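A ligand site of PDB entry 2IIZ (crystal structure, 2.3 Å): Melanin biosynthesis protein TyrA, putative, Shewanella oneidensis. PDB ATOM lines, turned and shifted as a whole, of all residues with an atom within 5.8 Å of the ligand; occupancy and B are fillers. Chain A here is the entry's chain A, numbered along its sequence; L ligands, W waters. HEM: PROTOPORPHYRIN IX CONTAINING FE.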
ATOM      1  N   ASP A 146     -18.065   5.019  -9.433  1.00  0.00           N
ATOM      2  CA  ASP A 146     -18.840   6.046  -8.743  1.00  0.00           C
ATOM      3  C   ASP A 146     -20.065   5.320  -8.264  1.00  0.00           C
ATOM      4  O   ASP A 146     -20.371   4.228  -8.766  1.00  0.00           O
ATOM      5  CB  ASP A 146     -19.200   7.161  -9.726  1.00  0.00           C
ATOM      6  CG  ASP A 146     -20.140   8.210  -9.137  1.00  0.00           C
ATOM      7  OD1 ASP A 146     -19.660   9.132  -8.445  1.00  0.00           O
ATOM      8  OD2 ASP A 146     -21.365   8.104  -9.378  1.00  0.00           O
ATOM      9  N   THR A 148     -22.995   5.764  -8.881  1.00  0.00           N
ATOM     10  CA  THR A 148     -23.878   5.538 -10.026  1.00  0.00           C
ATOM     11  C   THR A 148     -23.732   4.128 -10.650  1.00  0.00           C
ATOM     12  O   THR A 148     -24.599   3.679 -11.392  1.00  0.00           O
ATOM     13  CB  THR A 148     -23.693   6.603 -11.133  1.00  0.00           C
ATOM     14  OG1 THR A 148     -22.296   6.759 -11.455  1.00  0.00           O
ATOM     15  CG2 THR A 148     -24.186   7.924 -10.648  1.00  0.00           C
ATOM     16  N   PHE A 150     -21.043   3.318 -12.544  1.00  0.00           N
ATOM     17  CA  PHE A 150     -20.137   3.509 -13.697  1.00  0.00           C
ATOM     18  C   PHE A 150     -18.715   3.746 -13.246  1.00  0.00           C
ATOM     19  O   PHE A 150     -18.485   4.428 -12.249  1.00  0.00           O
ATOM     20  CB  PHE A 150     -20.581   4.723 -14.518  1.00  0.00           C
ATOM     21  CG  PHE A 150     -21.808   4.486 -15.356  1.00  0.00           C
ATOM     22  CD1 PHE A 150     -23.061   4.437 -14.757  1.00  0.00           C
ATOM     23  CD2 PHE A 150     -21.704   4.310 -16.732  1.00  0.00           C
ATOM     24  CE1 PHE A 150     -24.187   4.207 -15.501  1.00  0.00           C
ATOM     25  CE2 PHE A 150     -22.846   4.084 -17.493  1.00  0.00           C
ATOM     26  CZ  PHE A 150     -24.080   4.029 -16.890  1.00  0.00           C
ATOM     27  N   VAL A 151     -17.747   3.197 -13.981  1.00  0.00           N
ATOM     28  CA  VAL A 151     -16.325   3.299 -13.651  1.00  0.00           C
ATOM     29  C   VAL A 151     -15.877   4.731 -13.822  1.00  0.00           C
ATOM     30  O   VAL A 151     -16.062   5.306 -14.882  1.00  0.00           O
ATOM     31  CB  VAL A 151     -15.458   2.385 -14.563  1.00  0.00           C
ATOM     32  CG1 VAL A 151     -13.942   2.583 -14.330  1.00  0.00           C
ATOM     33  CG2 VAL A 151     -15.807   0.912 -14.365  1.00  0.00           C
ATOM     34  N   ASP A 152     -15.284   5.309 -12.777  1.00  0.00           N
ATOM     35  CA  ASP A 152     -14.762   6.685 -12.821  1.00  0.00           C
ATOM     36  C   ASP A 152     -13.237   6.611 -12.830  1.00  0.00           C
ATOM     37  O   ASP A 152     -12.659   5.900 -11.980  1.00  0.00           O
ATOM     38  CB  ASP A 152     -15.230   7.469 -11.594  1.00  0.00           C
ATOM     39  CG  ASP A 152     -14.895   8.976 -11.662  1.00  0.00           C
ATOM     40  OD1 ASP A 152     -14.878   9.583 -12.765  1.00  0.00           O
ATOM     41  OD2 ASP A 152     -14.659   9.563 -10.588  1.00  0.00           O
ATOM     42  N   GLY A 153     -12.598   7.300 -13.779  1.00  0.00           N
ATOM     43  CA  GLY A 153     -11.117   7.403 -13.858  1.00  0.00           C
ATOM     44  C   GLY A 153     -10.470   7.096 -15.219  1.00  0.00           C
ATOM     45  O   GLY A 153      -9.309   7.444 -15.485  1.00  0.00           O
ATOM     46  N   THR A 154     -11.234   6.438 -16.080  1.00  0.00           N
ATOM     47  CA  THR A 154     -10.697   5.739 -17.234  1.00  0.00           C
ATOM     48  C   THR A 154      -9.792   6.607 -18.132  1.00  0.00           C
ATOM     49  O   THR A 154      -8.716   6.175 -18.503  1.00  0.00           O
ATOM     50  CB  THR A 154     -11.852   5.141 -18.027  1.00  0.00           C
ATOM     51  OG1 THR A 154     -12.576   4.236 -17.182  1.00  0.00           O
ATOM     52  CG2 THR A 154     -11.345   4.424 -19.277  1.00  0.00           C
ATOM     53  N   GLU A 155     -10.246   7.822 -18.465  1.00  0.00           N
ATOM     54  CA  GLU A 155      -9.519   8.675 -19.419  1.00  0.00           C
ATOM     55  C   GLU A 155      -8.612   9.708 -18.736  1.00  0.00           C
ATOM     56  O   GLU A 155      -8.157  10.667 -19.378  1.00  0.00           O
ATOM     57  CB  GLU A 155     -10.503   9.383 -20.340  1.00  0.00           C
ATOM     58  CG  GLU A 155     -11.134   8.450 -21.372  1.00  0.00           C
ATOM     59  CD  GLU A 155     -10.138   7.964 -22.412  1.00  0.00           C
ATOM     60  OE1 GLU A 155      -9.526   8.819 -23.103  1.00  0.00           O
ATOM     61  OE2 GLU A 155      -9.966   6.724 -22.546  1.00  0.00           O
ATOM     62  N   ASN A 156      -8.344   9.507 -17.446  1.00  0.00           N
ATOM     63  CA  ASN A 156      -7.311  10.285 -16.758  1.00  0.00           C
ATOM     64  C   ASN A 156      -5.952  10.127 -17.432  1.00  0.00           C
ATOM     65  O   ASN A 156      -5.667   9.092 -18.004  1.00  0.00           O
ATOM     66  CB  ASN A 156      -7.173   9.840 -15.288  1.00  0.00           C
ATOM     67  CG  ASN A 156      -7.756  10.854 -14.285  1.00  0.00           C
ATOM     68  OD1 ASN A 156      -8.257  11.920 -14.637  1.00  0.00           O
ATOM     69  ND2 ASN A 156      -7.658  10.495 -13.011  1.00  0.00           N
ATOM     70  N   GLN A 184     -15.435  19.880  -5.455  1.00  0.00           N
ATOM     71  CA  GLN A 184     -16.887  19.989  -5.425  1.00  0.00           C
ATOM     72  C   GLN A 184     -17.416  18.768  -4.700  1.00  0.00           C
ATOM     73  O   GLN A 184     -17.156  17.653  -5.116  1.00  0.00           O
ATOM     74  CB  GLN A 184     -17.484  20.006  -6.840  1.00  0.00           C
ATOM     75  CG  GLN A 184     -17.120  21.211  -7.682  1.00  0.00           C
ATOM     76  CD  GLN A 184     -18.059  21.354  -8.885  1.00  0.00           C
ATOM     77  OE1 GLN A 184     -17.841  20.729  -9.925  1.00  0.00           O
ATOM     78  NE2 GLN A 184     -19.112  22.171  -8.727  1.00  0.00           N
ATOM     79  N   TYR A 186     -20.272  16.595  -4.403  1.00  0.00           N
ATOM     80  CA  TYR A 186     -21.489  16.232  -5.132  1.00  0.00           C
ATOM     81  C   TYR A 186     -22.341  15.234  -4.340  1.00  0.00           C
ATOM     82  O   TYR A 186     -21.903  14.113  -4.035  1.00  0.00           O
ATOM     83  CB  TYR A 186     -21.158  15.645  -6.511  1.00  0.00           C
ATOM     84  CG  TYR A 186     -20.813  16.655  -7.601  1.00  0.00           C
ATOM     85  CD1 TYR A 186     -21.787  17.217  -8.389  1.00  0.00           C
ATOM     86  CD2 TYR A 186     -19.503  17.012  -7.844  1.00  0.00           C
ATOM     87  CE1 TYR A 186     -21.476  18.138  -9.402  1.00  0.00           C
ATOM     88  CE2 TYR A 186     -19.168  17.940  -8.854  1.00  0.00           C
ATOM     89  CZ  TYR A 186     -20.168  18.497  -9.631  1.00  0.00           C
ATOM     90  OH  TYR A 186     -19.868  19.400 -10.623  1.00  0.00           O
ATOM     91  N   HIS A 188     -25.357  12.911  -4.635  1.00  0.00           N
ATOM     92  CA  HIS A 188     -26.115  12.233  -5.673  1.00  0.00           C
ATOM     93  C   HIS A 188     -27.524  12.003  -5.143  1.00  0.00           C
ATOM     94  O   HIS A 188     -27.720  11.780  -3.938  1.00  0.00           O
ATOM     95  CB  HIS A 188     -25.492  10.866  -6.024  1.00  0.00           C
ATOM     96  CG  HIS A 188     -24.159  10.950  -6.693  1.00  0.00           C
ATOM     97  ND1 HIS A 188     -23.562  12.138  -7.057  1.00  0.00           N
ATOM     98  CD2 HIS A 188     -23.309   9.965  -7.095  1.00  0.00           C
ATOM     99  CE1 HIS A 188     -22.394  11.887  -7.636  1.00  0.00           C
ATOM    100  NE2 HIS A 188     -22.221  10.577  -7.676  1.00  0.00           N
ATOM    101  N   ILE A 205     -24.072   9.183 -19.433  1.00  0.00           N
ATOM    102  CA  ILE A 205     -22.616   9.188 -19.288  1.00  0.00           C
ATOM    103  C   ILE A 205     -21.876   9.135 -20.620  1.00  0.00           C
ATOM    104  O   ILE A 205     -20.855   9.789 -20.734  1.00  0.00           O
ATOM    105  CB  ILE A 205     -22.190   8.101 -18.319  1.00  0.00           C
ATOM    106  CG1 ILE A 205     -22.555   8.596 -16.921  1.00  0.00           C
ATOM    107  CG2 ILE A 205     -20.658   7.832 -18.427  1.00  0.00           C
ATOM    108  CD1 ILE A 205     -22.842   7.541 -15.989  1.00  0.00           C
ATOM    109  N   ARG A 207     -20.950   6.103 -21.959  1.00  0.00           N
ATOM    110  CA  ARG A 207     -20.238   4.823 -21.953  1.00  0.00           C
ATOM    111  C   ARG A 207     -21.201   3.725 -21.484  1.00  0.00           C
ATOM    112  O   ARG A 207     -22.171   4.025 -20.787  1.00  0.00           O
ATOM    113  CB  ARG A 207     -19.032   4.892 -21.027  1.00  0.00           C
ATOM    114  CG  ARG A 207     -18.083   6.041 -21.338  1.00  0.00           C
ATOM    115  CD  ARG A 207     -16.947   6.086 -20.370  1.00  0.00           C
ATOM    116  NE  ARG A 207     -15.963   5.062 -20.645  1.00  0.00           N
ATOM    117  CZ  ARG A 207     -14.859   5.231 -21.368  1.00  0.00           C
ATOM    118  NH1 ARG A 207     -14.566   6.403 -21.915  1.00  0.00           N
ATOM    119  NH2 ARG A 207     -14.043   4.211 -21.555  1.00  0.00           N
ATOM    120  N   ASN A 212     -17.963  -0.795 -19.578  1.00  0.00           N
ATOM    121  CA  ASN A 212     -17.348   0.532 -19.631  1.00  0.00           C
ATOM    122  C   ASN A 212     -16.753   0.860 -20.986  1.00  0.00           C
ATOM    123  O   ASN A 212     -15.600   1.250 -21.085  1.00  0.00           O
ATOM    124  CB  ASN A 212     -16.266   0.669 -18.560  1.00  0.00           C
ATOM    125  CG  ASN A 212     -15.727   2.084 -18.454  1.00  0.00           C
ATOM    126  OD1 ASN A 212     -16.443   3.086 -18.754  1.00  0.00           O
ATOM    127  ND2 ASN A 212     -14.464   2.196 -18.014  1.00  0.00           N
ATOM    128  N   GLU A 214     -16.544   3.028 -24.325  1.00  0.00           N
ATOM    129  CA  GLU A 214     -16.812   4.373 -24.780  1.00  0.00           C
ATOM    130  C   GLU A 214     -17.679   4.301 -26.012  1.00  0.00           C
ATOM    131  O   GLU A 214     -17.381   3.522 -26.906  1.00  0.00           O
ATOM    132  CB  GLU A 214     -15.501   5.110 -25.073  1.00  0.00           C
ATOM    133  CG  GLU A 214     -15.679   6.592 -25.471  1.00  0.00           C
ATOM    134  CD  GLU A 214     -14.368   7.397 -25.491  1.00  0.00           C
ATOM    135  OE1 GLU A 214     -13.266   6.815 -25.437  1.00  0.00           O
ATOM    136  OE2 GLU A 214     -14.461   8.641 -25.589  1.00  0.00           O
ATOM    137  N   LYS A 220     -22.378   9.265 -29.331  1.00  0.00           N
ATOM    138  CA  LYS A 220     -22.371  10.113 -28.115  1.00  0.00           C
ATOM    139  C   LYS A 220     -23.425  11.215 -28.220  1.00  0.00           C
ATOM    140  O   LYS A 220     -23.332  12.070 -29.117  1.00  0.00           O
ATOM    141  CB  LYS A 220     -21.000  10.790 -27.895  1.00  0.00           C
ATOM    142  CG  LYS A 220     -19.918   9.935 -27.237  1.00  0.00           C
ATOM    143  CD  LYS A 220     -18.588  10.688 -27.111  1.00  0.00           C
ATOM    144  CE  LYS A 220     -17.430   9.755 -26.699  1.00  0.00           C
ATOM    145  NZ  LYS A 220     -16.231  10.480 -26.180  1.00  0.00           N
ATOM    146  N   HIS A 225     -22.320  13.282 -20.333  1.00  0.00           N
ATOM    147  CA  HIS A 225     -21.197  13.765 -19.524  1.00  0.00           C
ATOM    148  C   HIS A 225     -19.868  13.853 -20.274  1.00  0.00           C
ATOM    149  O   HIS A 225     -19.189  14.872 -20.203  1.00  0.00           O
ATOM    150  CB  HIS A 225     -20.989  12.900 -18.262  1.00  0.00           C
ATOM    151  CG  HIS A 225     -20.042  13.508 -17.273  1.00  0.00           C
ATOM    152  ND1 HIS A 225     -20.029  14.850 -16.969  1.00  0.00           N
ATOM    153  CD2 HIS A 225     -19.085  12.943 -16.509  1.00  0.00           C
ATOM    154  CE1 HIS A 225     -19.092  15.089 -16.077  1.00  0.00           C
ATOM    155  NE2 HIS A 225     -18.500  13.951 -15.767  1.00  0.00           N
ATOM    156  N   ILE A 226     -19.498  12.787 -20.995  1.00  0.00           N
ATOM    157  CA  ILE A 226     -18.199  12.642 -21.673  1.00  0.00           C
ATOM    158  C   ILE A 226     -18.082  13.504 -22.948  1.00  0.00           C
ATOM    159  O   ILE A 226     -16.965  13.843 -23.392  1.00  0.00           O
ATOM    160  CB  ILE A 226     -17.948  11.155 -22.091  1.00  0.00           C
ATOM    161  CG1 ILE A 226     -18.094  10.224 -20.899  1.00  0.00           C
ATOM    162  CG2 ILE A 226     -16.583  10.918 -22.662  1.00  0.00           C
ATOM    163  CD1 ILE A 226     -17.434  10.713 -19.690  1.00  0.00           C
ATOM    164  N   VAL A 229     -17.500  17.228 -21.354  1.00  0.00           N
ATOM    165  CA  VAL A 229     -16.228  17.509 -20.665  1.00  0.00           C
ATOM    166  C   VAL A 229     -14.970  17.044 -21.414  1.00  0.00           C
ATOM    167  O   VAL A 229     -13.864  17.105 -20.871  1.00  0.00           O
ATOM    168  CB  VAL A 229     -16.195  16.850 -19.253  1.00  0.00           C
ATOM    169  CG1 VAL A 229     -17.347  17.344 -18.389  1.00  0.00           C
ATOM    170  CG2 VAL A 229     -16.229  15.352 -19.391  1.00  0.00           C
ATOM    171  N   ASN A 230     -15.126  16.570 -22.646  1.00  0.00           N
ATOM    172  CA  ASN A 230     -13.986  16.364 -23.544  1.00  0.00           C
ATOM    173  C   ASN A 230     -13.942  17.540 -24.506  1.00  0.00           C
ATOM    174  O   ASN A 230     -14.715  17.593 -25.456  1.00  0.00           O
ATOM    175  CB  ASN A 230     -14.077  15.052 -24.324  1.00  0.00           C
ATOM    176  CG  ASN A 230     -12.826  14.794 -25.170  1.00  0.00           C
ATOM    177  OD1 ASN A 230     -12.598  15.467 -26.190  1.00  0.00           O
ATOM    178  ND2 ASN A 230     -12.018  13.811 -24.757  1.00  0.00           N
ATOM    179  N   ILE A 239      -7.713  19.521 -23.870  1.00  0.00           N
ATOM    180  CA  ILE A 239      -7.683  20.287 -22.641  1.00  0.00           C
ATOM    181  C   ILE A 239      -7.973  19.304 -21.517  1.00  0.00           C
ATOM    182  O   ILE A 239      -9.117  18.838 -21.379  1.00  0.00           O
ATOM    183  CB  ILE A 239      -8.779  21.362 -22.692  1.00  0.00           C
ATOM    184  CG2 ILE A 239      -8.734  22.257 -21.476  1.00  0.00           C
ATOM    185  N   ILE A 241      -7.464  17.483 -17.397  1.00  0.00           N
ATOM    186  CA  ILE A 241      -7.207  17.617 -15.966  1.00  0.00           C
ATOM    187  C   ILE A 241      -6.898  16.241 -15.394  1.00  0.00           C
ATOM    188  O   ILE A 241      -7.196  15.199 -16.014  1.00  0.00           O
ATOM    189  CB  ILE A 241      -8.399  18.225 -15.194  1.00  0.00           C
ATOM    190  CG1 ILE A 241      -9.680  17.438 -15.460  1.00  0.00           C
ATOM    191  CG2 ILE A 241      -8.603  19.681 -15.557  1.00  0.00           C
ATOM    192  CD1 ILE A 241     -10.628  17.450 -14.286  1.00  0.00           C
ATOM    193  N   ARG A 243      -8.027  14.099 -12.412  1.00  0.00           N
ATOM    194  CA  ARG A 243      -8.987  13.998 -11.321  1.00  0.00           C
ATOM    195  C   ARG A 243      -8.515  13.010 -10.306  1.00  0.00           C
ATOM    196  O   ARG A 243      -7.888  12.012 -10.633  1.00  0.00           O
ATOM    197  CB  ARG A 243     -10.319  13.507 -11.852  1.00  0.00           C
ATOM    198  CG  ARG A 243     -11.045  14.503 -12.707  1.00  0.00           C
ATOM    199  CD  ARG A 243     -12.102  13.758 -13.489  1.00  0.00           C
ATOM    200  NE  ARG A 243     -11.487  12.983 -14.572  1.00  0.00           N
ATOM    201  CZ  ARG A 243     -11.958  11.851 -15.073  1.00  0.00           C
ATOM    202  NH1 ARG A 243     -13.068  11.280 -14.579  1.00  0.00           N
ATOM    203  NH2 ARG A 243     -11.299  11.262 -16.054  1.00  0.00           N
ATOM    204  N   LEU A 256     -20.074  11.964  -4.826  1.00  0.00           N
ATOM    205  CA  LEU A 256     -18.710  12.042  -5.281  1.00  0.00           C
ATOM    206  C   LEU A 256     -18.024  13.252  -4.697  1.00  0.00           C
ATOM    207  O   LEU A 256     -18.557  14.378  -4.729  1.00  0.00           O
ATOM    208  CB  LEU A 256     -18.653  12.166  -6.821  1.00  0.00           C
ATOM    209  CG  LEU A 256     -17.250  11.997  -7.414  1.00  0.00           C
ATOM    210  CD1 LEU A 256     -16.861  10.551  -7.311  1.00  0.00           C
ATOM    211  CD2 LEU A 256     -17.130  12.450  -8.866  1.00  0.00           C
ATOM    212  N   PHE A 258     -15.616  15.350  -5.799  1.00  0.00           N
ATOM    213  CA  PHE A 258     -14.916  15.703  -6.988  1.00  0.00           C
ATOM    214  C   PHE A 258     -13.711  16.576  -6.730  1.00  0.00           C
ATOM    215  O   PHE A 258     -13.830  17.652  -6.115  1.00  0.00           O
ATOM    216  CB  PHE A 258     -15.784  16.410  -8.006  1.00  0.00           C
ATOM    217  CG  PHE A 258     -15.060  16.705  -9.257  1.00  0.00           C
ATOM    218  CD1 PHE A 258     -15.020  15.770 -10.262  1.00  0.00           C
ATOM    219  CD2 PHE A 258     -14.401  17.913  -9.412  1.00  0.00           C
ATOM    220  CE1 PHE A 258     -14.334  16.023 -11.442  1.00  0.00           C
ATOM    221  CE2 PHE A 258     -13.708  18.195 -10.581  1.00  0.00           C
ATOM    222  CZ  PHE A 258     -13.668  17.243 -11.612  1.00  0.00           C
ATOM    223  N   PHE A 268     -10.529  23.121 -15.634  1.00  0.00           N
ATOM    224  CA  PHE A 268     -11.742  22.760 -14.856  1.00  0.00           C
ATOM    225  C   PHE A 268     -12.903  23.717 -15.157  1.00  0.00           C
ATOM    226  O   PHE A 268     -14.034  23.282 -15.302  1.00  0.00           O
ATOM    227  CB  PHE A 268     -11.432  22.766 -13.367  1.00  0.00           C
ATOM    228  CG  PHE A 268     -12.652  22.828 -12.473  1.00  0.00           C
ATOM    229  CD1 PHE A 268     -13.332  21.669 -12.125  1.00  0.00           C
ATOM    230  CD2 PHE A 268     -13.123  24.037 -11.971  1.00  0.00           C
ATOM    231  CE1 PHE A 268     -14.455  21.722 -11.301  1.00  0.00           C
ATOM    232  CE2 PHE A 268     -14.242  24.096 -11.155  1.00  0.00           C
ATOM    233  CZ  PHE A 268     -14.898  22.935 -10.825  1.00  0.00           C
ATOM    234  N   MET A 271     -14.572  23.199 -18.490  1.00  0.00           N
ATOM    235  CA  MET A 271     -15.356  21.964 -18.402  1.00  0.00           C
ATOM    236  C   MET A 271     -16.652  22.187 -17.661  1.00  0.00           C
ATOM    237  O   MET A 271     -17.691  21.755 -18.101  1.00  0.00           O
ATOM    238  CB  MET A 271     -14.579  20.844 -17.691  1.00  0.00           C
ATOM    239  CG  MET A 271     -13.584  20.147 -18.599  1.00  0.00           C
ATOM    240  SD  MET A 271     -12.213  19.194 -17.610  1.00  0.00           S
ATOM    241  CE  MET A 271     -11.243  18.507 -19.028  1.00  0.00           C
ATOM    242  N   LEU A 272     -16.581  22.887 -16.533  1.00  0.00           N
ATOM    243  CA  LEU A 272     -17.747  23.128 -15.716  1.00  0.00           C
ATOM    244  C   LEU A 272     -18.765  24.002 -16.452  1.00  0.00           C
ATOM    245  O   LEU A 272     -19.975  23.755 -16.414  1.00  0.00           O
ATOM    246  CB  LEU A 272     -17.329  23.775 -14.426  1.00  0.00           C
ATOM    247  CG  LEU A 272     -18.427  23.960 -13.389  1.00  0.00           C
ATOM    248  CD1 LEU A 272     -18.849  22.617 -12.821  1.00  0.00           C
ATOM    249  CD2 LEU A 272     -17.979  24.948 -12.263  1.00  0.00           C
ATOM    250  N   MET A 275     -20.516  21.947 -18.817  1.00  0.00           N
ATOM    251  CA  MET A 275     -21.502  21.095 -18.135  1.00  0.00           C
ATOM    252  C   MET A 275     -22.782  21.847 -17.754  1.00  0.00           C
ATOM    253  O   MET A 275     -23.879  21.378 -18.019  1.00  0.00           O
ATOM    254  CB  MET A 275     -20.919  20.489 -16.857  1.00  0.00           C
ATOM    255  CG  MET A 275     -19.728  19.584 -17.048  1.00  0.00           C
ATOM    256  SD  MET A 275     -19.134  18.814 -15.403  1.00  0.00           S
ATOM    257  CE  MET A 275     -20.719  18.532 -14.507  1.00  0.00           C
ATOM    258  N   LEU A 287     -26.252  14.637 -16.594  1.00  0.00           N
ATOM    259  CA  LEU A 287     -25.817  13.984 -15.355  1.00  0.00           C
ATOM    260  C   LEU A 287     -26.176  14.891 -14.197  1.00  0.00           C
ATOM    261  O   LEU A 287     -26.491  14.428 -13.078  1.00  0.00           O
ATOM    262  CB  LEU A 287     -24.310  13.699 -15.365  1.00  0.00           C
ATOM    263  CG  LEU A 287     -23.708  13.001 -14.124  1.00  0.00           C
ATOM    264  CD1 LEU A 287     -24.451  11.721 -13.780  1.00  0.00           C
ATOM    265  CD2 LEU A 287     -22.216  12.688 -14.327  1.00  0.00           C
ATOM    266  N   THR A 291     -27.493  14.808  -9.476  1.00  0.00           N
ATOM    267  CA  THR A 291     -26.604  15.098  -8.359  1.00  0.00           C
ATOM    268  C   THR A 291     -26.504  16.582  -8.202  1.00  0.00           C
ATOM    269  O   THR A 291     -26.710  17.305  -9.167  1.00  0.00           O
ATOM    270  CB  THR A 291     -25.214  14.526  -8.599  1.00  0.00           C
ATOM    271  OG1 THR A 291     -24.442  14.622  -7.392  1.00  0.00           O
ATOM    272  CG2 THR A 291     -24.520  15.237  -9.737  1.00  0.00           C
HETATM  273  CHA HEM L   1     -15.294  11.395 -17.259  1.00  0.00           C
HETATM  274  CHB HEM L   1     -18.303  10.710 -13.560  1.00  0.00           C
HETATM  275  CHC HEM L   1     -18.037  15.340 -12.386  1.00  0.00           C
HETATM  276  CHD HEM L   1     -14.618  15.940 -15.700  1.00  0.00           C
HETATM  277  C1A HEM L   1     -16.163  10.814 -16.373  1.00  0.00           C
HETATM  278  C2A HEM L   1     -16.615   9.431 -16.425  1.00  0.00           C
HETATM  279  C3A HEM L   1     -17.449   9.260 -15.385  1.00  0.00           C
HETATM  280  C4A HEM L   1     -17.538  10.512 -14.669  1.00  0.00           C
HETATM  281  CMA HEM L   1     -18.211   7.982 -14.994  1.00  0.00           C
HETATM  282  CAA HEM L   1     -16.189   8.394 -17.493  1.00  0.00           C
HETATM  283  CBA HEM L   1     -14.936   7.601 -17.045  1.00  0.00           C
HETATM  284  CGA HEM L   1     -13.680   8.423 -17.242  1.00  0.00           C
HETATM  285  O1A HEM L   1     -13.087   8.895 -16.214  1.00  0.00           O
HETATM  286  O2A HEM L   1     -13.247   8.609 -18.404  1.00  0.00           O
HETATM  287  C1B HEM L   1     -18.500  11.905 -12.941  1.00  0.00           C
HETATM  288  C2B HEM L   1     -19.380  12.122 -11.816  1.00  0.00           C
HETATM  289  C3B HEM L   1     -19.305  13.414 -11.482  1.00  0.00           C
HETATM  290  C4B HEM L   1     -18.372  14.038 -12.399  1.00  0.00           C
HETATM  291  CMB HEM L   1     -20.227  10.994 -11.167  1.00  0.00           C
HETATM  292  CAB HEM L   1     -20.029  14.199 -10.375  1.00  0.00           C
HETATM  293  CBB HEM L   1     -21.260  13.888 -10.017  1.00  0.00           C
HETATM  294  C1C HEM L   1     -17.104  15.895 -13.208  1.00  0.00           C
HETATM  295  C2C HEM L   1     -16.755  17.296 -13.203  1.00  0.00           C
HETATM  296  C3C HEM L   1     -15.810  17.480 -14.126  1.00  0.00           C
HETATM  297  C4C HEM L   1     -15.534  16.184 -14.720  1.00  0.00           C
HETATM  298  CMC HEM L   1     -17.426  18.323 -12.274  1.00  0.00           C
HETATM  299  CAC HEM L   1     -15.095  18.774 -14.527  1.00  0.00           C
HETATM  300  CBC HEM L   1     -15.354  19.985 -14.006  1.00  0.00           C
HETATM  301  C1D HEM L   1     -14.466  14.779 -16.409  1.00  0.00           C
HETATM  302  C2D HEM L   1     -13.480  14.582 -17.440  1.00  0.00           C
HETATM  303  C3D HEM L   1     -13.687  13.163 -17.924  1.00  0.00           C
HETATM  304  C4D HEM L   1     -14.779  12.655 -17.140  1.00  0.00           C
HETATM  305  CMD HEM L   1     -12.438  15.612 -17.939  1.00  0.00           C
HETATM  306  CAD HEM L   1     -12.921  12.408 -19.028  1.00  0.00           C
HETATM  307  CBD HEM L   1     -13.723  12.528 -20.308  1.00  0.00           C
HETATM  308  CGD HEM L   1     -12.935  12.091 -21.516  1.00  0.00           C
HETATM  309  O1D HEM L   1     -13.231  10.977 -22.056  1.00  0.00           O
HETATM  310  O2D HEM L   1     -12.032  12.851 -21.941  1.00  0.00           O
HETATM  311  NA  HEM L   1     -16.750  11.452 -15.292  1.00  0.00           N
HETATM  312  NB  HEM L   1     -17.895  13.098 -13.283  1.00  0.00           N
HETATM  313  NC  HEM L   1     -16.343  15.227 -14.135  1.00  0.00           N
HETATM  314  ND  HEM L   1     -15.211  13.631 -16.260  1.00  0.00           N
HETATM  315 FE   HEM L   1     -16.715  13.380 -14.849  1.00  0.00          FE
HETATM  316  O   HOH W   1     -12.736  10.689 -24.567  1.00  0.00           O
HETATM  317  O   HOH W   2     -14.369   9.032 -20.698  1.00  0.00           O
HETATM  318  O   HOH W   3      -8.723  12.414 -22.793  1.00  0.00           O
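Water W1 lies within hydrogen-bond range of an oxygen (O1D) of the ligand (2.6 Å), the side-chain carboxylate of Glu 214 (2.9 Å) and the side-chain amide nitrogen of Asn 230 (3.2 Å).
Water W2 bridges an oxygen (O2A) of the ligand and the guanidinium group (NH1) of Arg 207.
An iron atom (FE) of the ligand is bound by a ring nitrogen (NE2) of His 225 (2.1 Å).
O1A of the ligand lies within salt-bridge range of NH1 of Arg 243 (2.9 Å).
The backbone NH (N) of Gly 153 sits at hydrogen-bond distance from an oxygen (O1A) of the ligand (3.0 Å).
O2D of the ligand is in hydrogen-bond range of ND2 of Asn 230.
The backbone NH of Thr 154 lies within hydrogen-bond range of an oxygen (O1A) of the ligand, 3.1 Å away.
An oxygen (O2A) of the ligand is in hydrogen-bond range of the backbone NH (N) of Glu 155 (3.1 Å).
The backbone carbonyl oxygen (O) of Arg 243 lies within hydrogen-bond range of the side-chain amide nitrogen (ND2) of Asn 156, 2.8 Å away.
The side-chain hydroxyl of Thr 154 lies within hydrogen-bond range of the side-chain amide nitrogen of Asn 212, at 2.9 Å.
OE1 of Gln 184 sits at hydrogen-bond distance from OH of Tyr 186.
O of Phe 258 is in hydrogen-bond range of N of Gln 184 (2.8 Å).
NE2 of His 188 is in hydrogen-bond range of OD1 of Asp 146.
The side-chain carboxylate of Asp 146 is in hydrogen-bond range of the side-chain hydroxyl of Thr 148 (2.6 Å).
OE1 of Glu 214 is in salt-bridge range of NH1 of Arg 207 (3.8 Å).
The side-chain amide oxygen of Asn 212 sits at hydrogen-bond distance from the guanidinium group of Arg 207, at 2.8 Å.
Merely in contact with the ligand: Tyr 186 (3.1 Å), Phe 268 (3.2 Å), Phe 258 (3.3 Å), Ile 226 (3.3 Å), His 188 (3.3 Å), Met 271 (3.3 Å), Asp 146 (3.3 Å), Val 151 (3.3 Å), Gln 184 (3.4 Å), Asp 152 (3.4 Å), Val 229 (3.5 Å), Leu 256 (3.5 Å), Thr 291 (3.5 Å), Met 275 (3.6 Å), Arg 207 (3.8 Å) and Leu 287 (3.8 Å).
Hydrophobic or aromatic side chains within 4 Å of the ligand: Tyr 186, His 188, His 225, Ile 226, Val 229, Leu 256, Phe 258, Phe 268, Met 271, Met 275 and Leu 287.
22 residues have an atom within 4 Å of the ligand: Asp 146, Val 151, Asp 152, Gly 153, Thr 154, Glu 155, Gln 184, Tyr 186, His 188, Arg 207, His 225, Ile 226, Val 229, Asn 230, Arg 243, Leu 256, Phe 258, Phe 268, Met 271, Met 275, Leu 287 and Thr 291.
Along chain A the residues within 4 Å of the ligand span positions 146 to 291.
The nearest printed residue that does not touch the ligand is Leu 272 (4.04 Å).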
